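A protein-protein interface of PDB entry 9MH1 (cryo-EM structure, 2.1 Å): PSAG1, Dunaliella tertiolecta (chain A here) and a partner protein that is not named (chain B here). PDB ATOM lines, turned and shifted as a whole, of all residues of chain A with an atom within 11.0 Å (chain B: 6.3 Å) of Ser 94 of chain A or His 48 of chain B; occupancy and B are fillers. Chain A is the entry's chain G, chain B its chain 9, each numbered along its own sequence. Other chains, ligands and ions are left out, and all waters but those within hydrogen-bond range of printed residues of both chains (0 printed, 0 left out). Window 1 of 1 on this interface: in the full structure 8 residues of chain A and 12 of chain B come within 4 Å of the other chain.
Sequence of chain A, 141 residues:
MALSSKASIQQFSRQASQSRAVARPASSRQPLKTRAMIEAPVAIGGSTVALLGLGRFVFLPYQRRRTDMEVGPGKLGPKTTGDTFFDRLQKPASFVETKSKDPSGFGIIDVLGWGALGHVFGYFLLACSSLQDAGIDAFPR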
ATOM      1  N   PHE A  85       8.007  13.289   6.412  1.00  0.00           N
ATOM      2  CA  PHE A  85       8.818  12.479   7.320  1.00  0.00           C
ATOM      3  C   PHE A  85      10.307  12.758   7.150  1.00  0.00           C
ATOM      4  O   PHE A  85      11.035  12.866   8.142  1.00  0.00           O
ATOM      5  CB  PHE A  85       8.521  10.994   7.103  1.00  0.00           C
ATOM      6  CG  PHE A  85       9.677  10.082   7.428  1.00  0.00           C
ATOM      7  CD1 PHE A  85      10.060   9.856   8.744  1.00  0.00           C
ATOM      8  CD2 PHE A  85      10.369   9.435   6.416  1.00  0.00           C
ATOM      9  CE1 PHE A  85      11.116   9.015   9.039  1.00  0.00           C
ATOM     10  CE2 PHE A  85      11.427   8.593   6.707  1.00  0.00           C
ATOM     11  CZ  PHE A  85      11.801   8.383   8.020  1.00  0.00           C
ATOM     12  N   ARG A  88      11.149  16.408   8.509  1.00  0.00           N
ATOM     13  CA  ARG A  88      11.242  16.459   9.963  1.00  0.00           C
ATOM     14  C   ARG A  88      12.303  15.513  10.511  1.00  0.00           C
ATOM     15  O   ARG A  88      12.713  15.664  11.667  1.00  0.00           O
ATOM     16  CB  ARG A  88       9.883  16.153  10.601  1.00  0.00           C
ATOM     17  CG  ARG A  88       9.396  14.730  10.416  1.00  0.00           C
ATOM     18  CD  ARG A  88       7.934  14.603  10.818  1.00  0.00           C
ATOM     19  NE  ARG A  88       7.049  15.383   9.961  1.00  0.00           N
ATOM     20  CZ  ARG A  88       6.017  16.090  10.400  1.00  0.00           C
ATOM     21  NH1 ARG A  88       5.708  16.137  11.686  1.00  0.00           N
ATOM     22  NH2 ARG A  88       5.276  16.767   9.528  1.00  0.00           N
ATOM     23  N   LEU A  89      12.747  14.539   9.714  1.00  0.00           N
ATOM     24  CA  LEU A  89      13.936  13.774  10.070  1.00  0.00           C
ATOM     25  C   LEU A  89      15.183  14.637   9.972  1.00  0.00           C
ATOM     26  O   LEU A  89      16.118  14.475  10.765  1.00  0.00           O
ATOM     27  CB  LEU A  89      14.060  12.546   9.169  1.00  0.00           C
ATOM     28  CG  LEU A  89      15.100  11.497   9.567  1.00  0.00           C
ATOM     29  CD1 LEU A  89      14.828  10.989  10.972  1.00  0.00           C
ATOM     30  CD2 LEU A  89      15.112  10.348   8.571  1.00  0.00           C
ATOM     31  N   GLN A  90      15.213  15.552   8.999  1.00  0.00           N
ATOM     32  CA  GLN A  90      16.258  16.567   8.954  1.00  0.00           C
ATOM     33  C   GLN A  90      16.177  17.509  10.149  1.00  0.00           C
ATOM     34  O   GLN A  90      17.203  18.039  10.589  1.00  0.00           O
ATOM     35  CB  GLN A  90      16.151  17.366   7.658  1.00  0.00           C
ATOM     36  CG  GLN A  90      17.004  16.860   6.517  1.00  0.00           C
ATOM     37  CD  GLN A  90      17.273  17.942   5.492  1.00  0.00           C
ATOM     38  OE1 GLN A  90      16.464  18.176   4.597  1.00  0.00           O
ATOM     39  NE2 GLN A  90      18.408  18.618   5.626  1.00  0.00           N
ATOM     40  N   LYS A  91      14.971  17.741  10.665  1.00  0.00           N
ATOM     41  CA  LYS A  91      14.789  18.623  11.809  1.00  0.00           C
ATOM     42  C   LYS A  91      15.437  18.015  13.053  1.00  0.00           C
ATOM     43  O   LYS A  91      15.368  16.798  13.254  1.00  0.00           O
ATOM     44  CB  LYS A  91      13.297  18.864  12.054  1.00  0.00           C
ATOM     45  CG  LYS A  91      12.974  19.891  13.127  1.00  0.00           C
ATOM     46  CD  LYS A  91      11.475  19.996  13.353  1.00  0.00           C
ATOM     47  CE  LYS A  91      11.152  20.963  14.480  1.00  0.00           C
ATOM     48  NZ  LYS A  91       9.688  21.031  14.750  1.00  0.00           N
ATOM     49  N   PRO A  92      16.103  18.826  13.877  1.00  0.00           N
ATOM     50  CA  PRO A  92      16.681  18.307  15.123  1.00  0.00           C
ATOM     51  C   PRO A  92      15.619  17.751  16.060  1.00  0.00           C
ATOM     52  O   PRO A  92      14.501  18.264  16.140  1.00  0.00           O
ATOM     53  CB  PRO A  92      17.373  19.533  15.728  1.00  0.00           C
ATOM     54  CG  PRO A  92      17.681  20.399  14.561  1.00  0.00           C
ATOM     55  CD  PRO A  92      16.548  20.203  13.596  1.00  0.00           C
ATOM     56  N   ALA A  93      15.984  16.688  16.772  1.00  0.00           N
ATOM     57  CA  ALA A  93      15.078  16.070  17.725  1.00  0.00           C
ATOM     58  C   ALA A  93      14.975  16.921  18.989  1.00  0.00           C
ATOM     59  O   ALA A  93      15.662  17.932  19.153  1.00  0.00           O
ATOM     60  CB  ALA A  93      15.544  14.656  18.068  1.00  0.00           C
ATOM     61  N   SER A  94      14.091  16.497  19.894  1.00  0.00           N
ATOM     62  CA  SER A  94      13.860  17.191  21.156  1.00  0.00           C
ATOM     63  C   SER A  94      14.678  16.611  22.302  1.00  0.00           C
ATOM     64  O   SER A  94      14.242  16.662  23.460  1.00  0.00           O
ATOM     65  CB  SER A  94      12.372  17.164  21.502  1.00  0.00           C
ATOM     66  OG  SER A  94      11.968  15.860  21.883  1.00  0.00           O
ATOM     67  N   PHE A  95      15.852  16.056  22.011  1.00  0.00           N
ATOM     68  CA  PHE A  95      16.667  15.379  23.010  1.00  0.00           C
ATOM     69  C   PHE A  95      17.982  16.087  23.305  1.00  0.00           C
ATOM     70  O   PHE A  95      18.450  16.043  24.445  1.00  0.00           O
ATOM     71  CB  PHE A  95      16.937  13.934  22.558  1.00  0.00           C
ATOM     72  CG  PHE A  95      18.170  13.311  23.151  1.00  0.00           C
ATOM     73  CD1 PHE A  95      18.180  12.874  24.467  1.00  0.00           C
ATOM     74  CD2 PHE A  95      19.308  13.126  22.381  1.00  0.00           C
ATOM     75  CE1 PHE A  95      19.309  12.292  25.009  1.00  0.00           C
ATOM     76  CE2 PHE A  95      20.439  12.545  22.917  1.00  0.00           C
ATOM     77  CZ  PHE A  95      20.438  12.125  24.231  1.00  0.00           C
ATOM     78  N   VAL A  96      18.570  16.769  22.317  1.00  0.00           N
ATOM     79  CA  VAL A  96      19.892  17.368  22.488  1.00  0.00           C
ATOM     80  C   VAL A  96      19.850  18.805  22.994  1.00  0.00           C
ATOM     81  O   VAL A  96      20.901  19.347  23.369  1.00  0.00           O
ATOM     82  CB  VAL A  96      20.683  17.322  21.164  1.00  0.00           C
ATOM     83  CG1 VAL A  96      20.527  15.964  20.501  1.00  0.00           C
ATOM     84  CG2 VAL A  96      20.226  18.427  20.222  1.00  0.00           C
ATOM     85  N   GLU A  97      18.674  19.442  23.024  1.00  0.00           N
ATOM     86  CA  GLU A  97      18.605  20.862  23.354  1.00  0.00           C
ATOM     87  C   GLU A  97      17.418  21.204  24.253  1.00  0.00           C
ATOM     88  O   GLU A  97      17.079  22.388  24.387  1.00  0.00           O
ATOM     89  CB  GLU A  97      18.555  21.708  22.062  1.00  0.00           C
ATOM     90  CG  GLU A  97      17.214  21.776  21.271  1.00  0.00           C
ATOM     91  CD  GLU A  97      16.463  20.452  21.083  1.00  0.00           C
ATOM     92  OE1 GLU A  97      15.246  20.515  20.803  1.00  0.00           O
ATOM     93  OE2 GLU A  97      17.072  19.362  21.128  1.00  0.00           O
ATOM     94  N   THR A  98      16.789  20.205  24.880  1.00  0.00           N
ATOM     95  CA  THR A  98      15.596  20.454  25.685  1.00  0.00           C
ATOM     96  C   THR A  98      15.912  21.313  26.905  1.00  0.00           C
ATOM     97  O   THR A  98      15.188  22.269  27.210  1.00  0.00           O
ATOM     98  CB  THR A  98      14.971  19.127  26.116  1.00  0.00           C
ATOM     99  OG1 THR A  98      14.988  18.210  25.016  1.00  0.00           O
ATOM    100  CG2 THR A  98      13.535  19.338  26.569  1.00  0.00           C
ATOM    101  N   LYS A  99      16.994  20.994  27.609  1.00  0.00           N
ATOM    102  CA  LYS A  99      17.366  21.711  28.822  1.00  0.00           C
ATOM    103  C   LYS A  99      18.834  21.437  29.116  1.00  0.00           C
ATOM    104  O   LYS A  99      19.447  20.533  28.544  1.00  0.00           O
ATOM    105  CB  LYS A  99      16.486  21.310  30.015  1.00  0.00           C
ATOM    106  CG  LYS A  99      16.920  20.033  30.727  1.00  0.00           C
ATOM    107  CD  LYS A  99      16.537  18.785  29.949  1.00  0.00           C
ATOM    108  CE  LYS A  99      17.200  17.553  30.524  1.00  0.00           C
ATOM    109  NZ  LYS A  99      17.124  16.404  29.584  1.00  0.00           N
ATOM    110  N   SER A 100      19.391  22.237  30.025  1.00  0.00           N
ATOM    111  CA  SER A 100      20.769  22.084  30.494  1.00  0.00           C
ATOM    112  C   SER A 100      20.736  22.126  32.018  1.00  0.00           C
ATOM    113  O   SER A 100      20.796  23.201  32.620  1.00  0.00           O
ATOM    114  CB  SER A 100      21.675  23.166  29.914  1.00  0.00           C
ATOM    115  OG  SER A 100      21.236  24.457  30.299  1.00  0.00           O
ATOM    116  N   ILE A 108      24.860  16.559  27.303  1.00  0.00           N
ATOM    117  CA  ILE A 108      25.424  15.219  27.198  1.00  0.00           C
ATOM    118  C   ILE A 108      26.027  14.948  25.824  1.00  0.00           C
ATOM    119  O   ILE A 108      26.870  14.055  25.703  1.00  0.00           O
ATOM    120  CB  ILE A 108      24.349  14.162  27.511  1.00  0.00           C
ATOM    121  CG1 ILE A 108      23.194  14.263  26.512  1.00  0.00           C
ATOM    122  CG2 ILE A 108      23.842  14.324  28.936  1.00  0.00           C
ATOM    123  CD1 ILE A 108      22.199  13.129  26.613  1.00  0.00           C
ATOM    124  N   ILE A 109      25.616  15.690  24.793  1.00  0.00           N
ATOM    125  CA  ILE A 109      26.282  15.590  23.497  1.00  0.00           C
ATOM    126  C   ILE A 109      27.721  16.081  23.583  1.00  0.00           C
ATOM    127  O   ILE A 109      28.642  15.433  23.067  1.00  0.00           O
ATOM    128  CB  ILE A 109      25.512  16.389  22.428  1.00  0.00           C
ATOM    129  CG1 ILE A 109      24.066  15.900  22.336  1.00  0.00           C
ATOM    130  CG2 ILE A 109      26.205  16.279  21.079  1.00  0.00           C
ATOM    131  CD1 ILE A 109      23.939  14.435  21.986  1.00  0.00           C
ATOM    132  N   ILE B  44      13.025  14.308  30.057  1.00  0.00           N
ATOM    133  CA  ILE B  44      13.281  14.478  28.627  1.00  0.00           C
ATOM    134  C   ILE B  44      11.976  14.221  27.882  1.00  0.00           C
ATOM    135  O   ILE B  44      11.780  13.121  27.344  1.00  0.00           O
ATOM    136  CB  ILE B  44      14.389  13.536  28.118  1.00  0.00           C
ATOM    137  CG1 ILE B  44      15.570  13.472  29.089  1.00  0.00           C
ATOM    138  CG2 ILE B  44      14.879  13.981  26.745  1.00  0.00           C
ATOM    139  CD1 ILE B  44      15.651  12.182  29.873  1.00  0.00           C
ATOM    140  N   PRO B  45      11.054  15.179  27.831  1.00  0.00           N
ATOM    141  CA  PRO B  45       9.754  14.926  27.202  1.00  0.00           C
ATOM    142  C   PRO B  45       9.792  15.201  25.709  1.00  0.00           C
ATOM    143  O   PRO B  45      10.140  16.310  25.278  1.00  0.00           O
ATOM    144  CB  PRO B  45       8.816  15.903  27.927  1.00  0.00           C
ATOM    145  CG  PRO B  45       9.710  17.011  28.423  1.00  0.00           C
ATOM    146  CD  PRO B  45      11.144  16.535  28.401  1.00  0.00           C
ATOM    147  N   PRO B  46       9.446  14.216  24.884  1.00  0.00           N
ATOM    148  CA  PRO B  46       9.341  14.455  23.444  1.00  0.00           C
ATOM    149  C   PRO B  46       7.919  14.815  23.052  1.00  0.00           C
ATOM    150  O   PRO B  46       6.953  14.360  23.683  1.00  0.00           O
ATOM    151  CB  PRO B  46       9.765  13.111  22.837  1.00  0.00           C
ATOM    152  CG  PRO B  46       9.350  12.103  23.861  1.00  0.00           C
ATOM    153  CD  PRO B  46       9.331  12.783  25.215  1.00  0.00           C
ATOM    154  N   PRO B  47       7.742  15.639  22.015  1.00  0.00           N
ATOM    155  CA  PRO B  47       6.383  16.004  21.592  1.00  0.00           C
ATOM    156  C   PRO B  47       5.749  14.975  20.667  1.00  0.00           C
ATOM    157  O   PRO B  47       4.520  14.877  20.594  1.00  0.00           O
ATOM    158  CB  PRO B  47       6.593  17.344  20.880  1.00  0.00           C
ATOM    159  CG  PRO B  47       7.977  17.255  20.332  1.00  0.00           C
ATOM    160  CD  PRO B  47       8.775  16.386  21.275  1.00  0.00           C
ATOM    161  N   HIS B  48       6.575  14.207  19.951  1.00  0.00           N
ATOM    162  CA  HIS B  48       6.041  13.235  19.002  1.00  0.00           C
ATOM    163  C   HIS B  48       5.432  12.036  19.717  1.00  0.00           C
ATOM    164  O   HIS B  48       4.430  11.474  19.257  1.00  0.00           O
ATOM    165  CB  HIS B  48       7.134  12.785  18.032  1.00  0.00           C
ATOM    166  CG  HIS B  48       8.490  12.675  18.656  1.00  0.00           C
ATOM    167  ND1 HIS B  48       9.354  13.744  18.753  1.00  0.00           N
ATOM    168  CD2 HIS B  48       9.135  11.619  19.207  1.00  0.00           C
ATOM    169  CE1 HIS B  48      10.471  13.354  19.342  1.00  0.00           C
ATOM    170  NE2 HIS B  48      10.364  12.068  19.626  1.00  0.00           N
ATOM    171  N   LEU B  49       6.018  11.627  20.837  1.00  0.00           N
ATOM    172  CA  LEU B  49       5.531  10.496  21.622  1.00  0.00           C
ATOM    173  C   LEU B  49       4.877  11.050  22.884  1.00  0.00           C
ATOM    174  O   LEU B  49       5.561  11.363  23.863  1.00  0.00           O
ATOM    175  CB  LEU B  49       6.667   9.530  21.949  1.00  0.00           C
ATOM    176  CG  LEU B  49       7.365   8.920  20.730  1.00  0.00           C
ATOM    177  CD1 LEU B  49       8.615   8.157  21.138  1.00  0.00           C
ATOM    178  CD2 LEU B  49       6.410   8.021  19.960  1.00  0.00           C
ATOM    179  N   ASN B  50       3.549  11.175  22.849  1.00  0.00           N
ATOM    180  CA  ASN B  50       2.823  11.721  23.992  1.00  0.00           C
ATOM    181  C   ASN B  50       2.816  10.749  25.166  1.00  0.00           C
ATOM    182  O   ASN B  50       2.960  11.163  26.322  1.00  0.00           O
ATOM    183  CB  ASN B  50       1.394  12.077  23.582  1.00  0.00           C
ATOM    184  CG  ASN B  50       0.761  11.018  22.700  1.00  0.00           C
ATOM    185  OD1 ASN B  50       1.385  10.007  22.377  1.00  0.00           O
ATOM    186  ND2 ASN B  50      -0.485  11.247  22.302  1.00  0.00           N
ATOM    187  N   GLY B  51       2.654   9.458  24.892  1.00  0.00           N
ATOM    188  CA  GLY B  51       2.630   8.464  25.947  1.00  0.00           C
ATOM    189  C   GLY B  51       1.455   7.514  25.851  1.00  0.00           C
ATOM    190  O   GLY B  51       1.252   6.677  26.735  1.00  0.00           O
ATOM    191  N   ASP B  56       5.390   3.559  26.572  1.00  0.00           N
ATOM    192  CA  ASP B  56       5.949   4.713  25.869  1.00  0.00           C
ATOM    193  C   ASP B  56       6.697   5.581  26.872  1.00  0.00           C
ATOM    194  O   ASP B  56       6.096   6.386  27.586  1.00  0.00           O
ATOM    195  CB  ASP B  56       4.848   5.498  25.165  1.00  0.00           C
ATOM    196  CG  ASP B  56       5.389   6.473  24.134  1.00  0.00           C
ATOM    197  OD1 ASP B  56       6.621   6.527  23.945  1.00  0.00           O
ATOM    198  OD2 ASP B  56       4.575   7.185  23.510  1.00  0.00           O
ATOM    199  N   GLY B  58       9.093   7.490  25.567  1.00  0.00           N
ATOM    200  CA  GLY B  58       9.604   8.525  24.689  1.00  0.00           C
ATOM    201  C   GLY B  58      11.039   8.336  24.254  1.00  0.00           C
ATOM    202  O   GLY B  58      11.724   9.322  23.963  1.00  0.00           O
ATOM    203  N   ASP B  60      13.268   8.196  21.914  1.00  0.00           N
ATOM    204  CA  ASP B  60      13.619   8.514  20.530  1.00  0.00           C
ATOM    205  C   ASP B  60      14.738   9.548  20.531  1.00  0.00           C
ATOM    206  O   ASP B  60      14.498  10.735  20.272  1.00  0.00           O
ATOM    207  CB  ASP B  60      12.401   9.018  19.752  1.00  0.00           C
ATOM    208  CG  ASP B  60      12.353   8.484  18.335  1.00  0.00           C
ATOM    209  OD1 ASP B  60      13.193   7.627  17.992  1.00  0.00           O
ATOM    210  OD2 ASP B  60      11.474   8.922  17.562  1.00  0.00           O
ATOM    211  N   PRO B  61      15.976   9.135  20.830  1.00  0.00           N
ATOM    212  CA  PRO B  61      17.079  10.112  20.792  1.00  0.00           C
ATOM    213  C   PRO B  61      17.437  10.552  19.386  1.00  0.00           C
ATOM    214  O   PRO B  61      17.713  11.738  19.165  1.00  0.00           O
ATOM    215  CB  PRO B  61      18.235   9.364  21.469  1.00  0.00           C
ATOM    216  CG  PRO B  61      17.928   7.928  21.272  1.00  0.00           C
ATOM    217  CD  PRO B  61      16.432   7.799  21.253  1.00  0.00           C
ATOM    218  N   GLY B  63      15.359  10.412  16.846  1.00  0.00           N
ATOM    219  CA  GLY B  63      14.147  10.781  16.141  1.00  0.00           C
ATOM    220  C   GLY B  63      13.764   9.802  15.051  1.00  0.00           C
ATOM    221  O   GLY B  63      13.475  10.204  13.920  1.00  0.00           O
ATOM    222  N   GLY B  65      11.093   7.612  14.969  1.00  0.00           N
ATOM    223  CA  GLY B  65       9.675   7.600  14.667  1.00  0.00           C
ATOM    224  C   GLY B  65       9.033   8.966  14.550  1.00  0.00           C
ATOM    225  O   GLY B  65       8.619   9.556  15.551  1.00  0.00           O
ATOM    226  N   LEU B  66       8.931   9.468  13.319  1.00  0.00           N
ATOM    227  CA  LEU B  66       8.228  10.715  13.031  1.00  0.00           C
ATOM    228  C   LEU B  66       7.322  10.640  11.812  1.00  0.00           C
ATOM    229  O   LEU B  66       6.659  11.636  11.509  1.00  0.00           O
ATOM    230  CB  LEU B  66       9.216  11.878  12.825  1.00  0.00           C
ATOM    231  CG  LEU B  66       9.883  12.679  13.955  1.00  0.00           C
ATOM    232  CD1 LEU B  66       8.833  13.420  14.779  1.00  0.00           C
ATOM    233  CD2 LEU B  66      10.816  11.874  14.847  1.00  0.00           C
ATOM    234  N   GLU B  68       4.557   8.986  11.212  1.00  0.00           N
ATOM    235  CA  GLU B  68       3.158   8.822  11.609  1.00  0.00           C
ATOM    236  C   GLU B  68       2.403   7.800  10.761  1.00  0.00           C
ATOM    237  O   GLU B  68       1.191   7.641  10.950  1.00  0.00           O
ATOM    238  CB  GLU B  68       2.377  10.146  11.601  1.00  0.00           C
ATOM    239  CG  GLU B  68       2.340  10.857  12.944  1.00  0.00           C
ATOM    240  CD  GLU B  68       3.714  11.301  13.409  1.00  0.00           C
ATOM    241  OE1 GLU B  68       4.152  12.400  13.009  1.00  0.00           O
ATOM    242  OE2 GLU B  68       4.353  10.554  14.180  1.00  0.00           O
ATOM    243  N   LEU B  71       5.485   4.512  11.748  1.00  0.00           N
ATOM    244  CA  LEU B  71       5.720   4.373  13.182  1.00  0.00           C
ATOM    245  C   LEU B  71       4.823   3.295  13.781  1.00  0.00           C
ATOM    246  O   LEU B  71       5.232   2.582  14.703  1.00  0.00           O
ATOM    247  CB  LEU B  71       5.509   5.714  13.886  1.00  0.00           C
ATOM    248  CG  LEU B  71       5.753   5.755  15.397  1.00  0.00           C
ATOM    249  CD1 LEU B  71       7.106   5.152  15.750  1.00  0.00           C
ATOM    250  CD2 LEU B  71       5.648   7.178  15.921  1.00  0.00           C
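Arg 88 of chain A touches Leu 66 of chain B. CD1 of Leu 89 of chain A touches O of Gly 63 of chain B, at 3.3 Å. CB of Ala 93 of chain A touches O of Pro 61 of chain B (3.8 Å). Ser 94 of chain A touches Pro 45 of chain B (OG to O, 3.9 Å). Ser 94 of chain A touches Pro 46 of chain B. Ser 94 of chain A touches Pro 47 of chain B (OG to CD, 3.3 Å). Ser 94 of chain A touches His 48 of chain B. Phe 95 of chain A touches Pro 61 of chain B (CD2 to O, 3.8 Å). Ile 44 of chain B touches Lys 99 of chain A (CG1 to NZ, 3.4 Å).
Printed residues of chain B that touch a printed residue of chain A: Ile 44, Pro 45, Pro 46, Pro 47, His 48, Pro 61, Gly 63 and Leu 66. Hydrophobic or aromatic side chains of chain B within 4 Å of the printed part of chain A: Ile 44, Pro 46, Pro 47, His 48 and Leu 66.
Printed residues of chain B within 4 Å of Arg 88 of chain A: Leu 66. Printed residues of chain B within 4 Å of Ala 93 of chain A: Pro 61 (3.8 Å). Of chain B, only Pro 45 (3.9 Å), Pro 46 (3.4 Å), Pro 47 (3.3 Å) and His 48 (3.9 Å) come within 4 Å of Ser 94 of chain A. Of the printed residues of chain B, Lys 99 of chain A touches Ile 44. Printed residues of chain A within 4 Å of Ile 44 of chain B: Lys 99 (3.4 Å). Pro 45 of chain B touches just one residue of chain A: Ser 94. Of chain A, only Ser 94 comes within 4 Å of Pro 46 of chain B. Of chain A, only Ser 94 (3.3 Å) comes within 4 Å of Pro 47 of chain B. Of the printed residues of chain A, His 48 of chain B touches Ser 94 (3.9 Å). No residue of chain A comes within 4 Å of Leu 49 of chain B. Asn 50 of chain B touches none of the printed residues of chain A. No residue of chain A comes within 4 Å of Asp 60 of chain B. No residue of chain A comes within 4 Å of Gly 65 of chain B. The nearest residue of chain A that does not touch His 48 of chain B is Ala 93 of chain A (5.4 Å). The nearest printed residue of chain B that does not touch Leu 89 of chain A is Leu 66 of chain B (5.4 Å).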
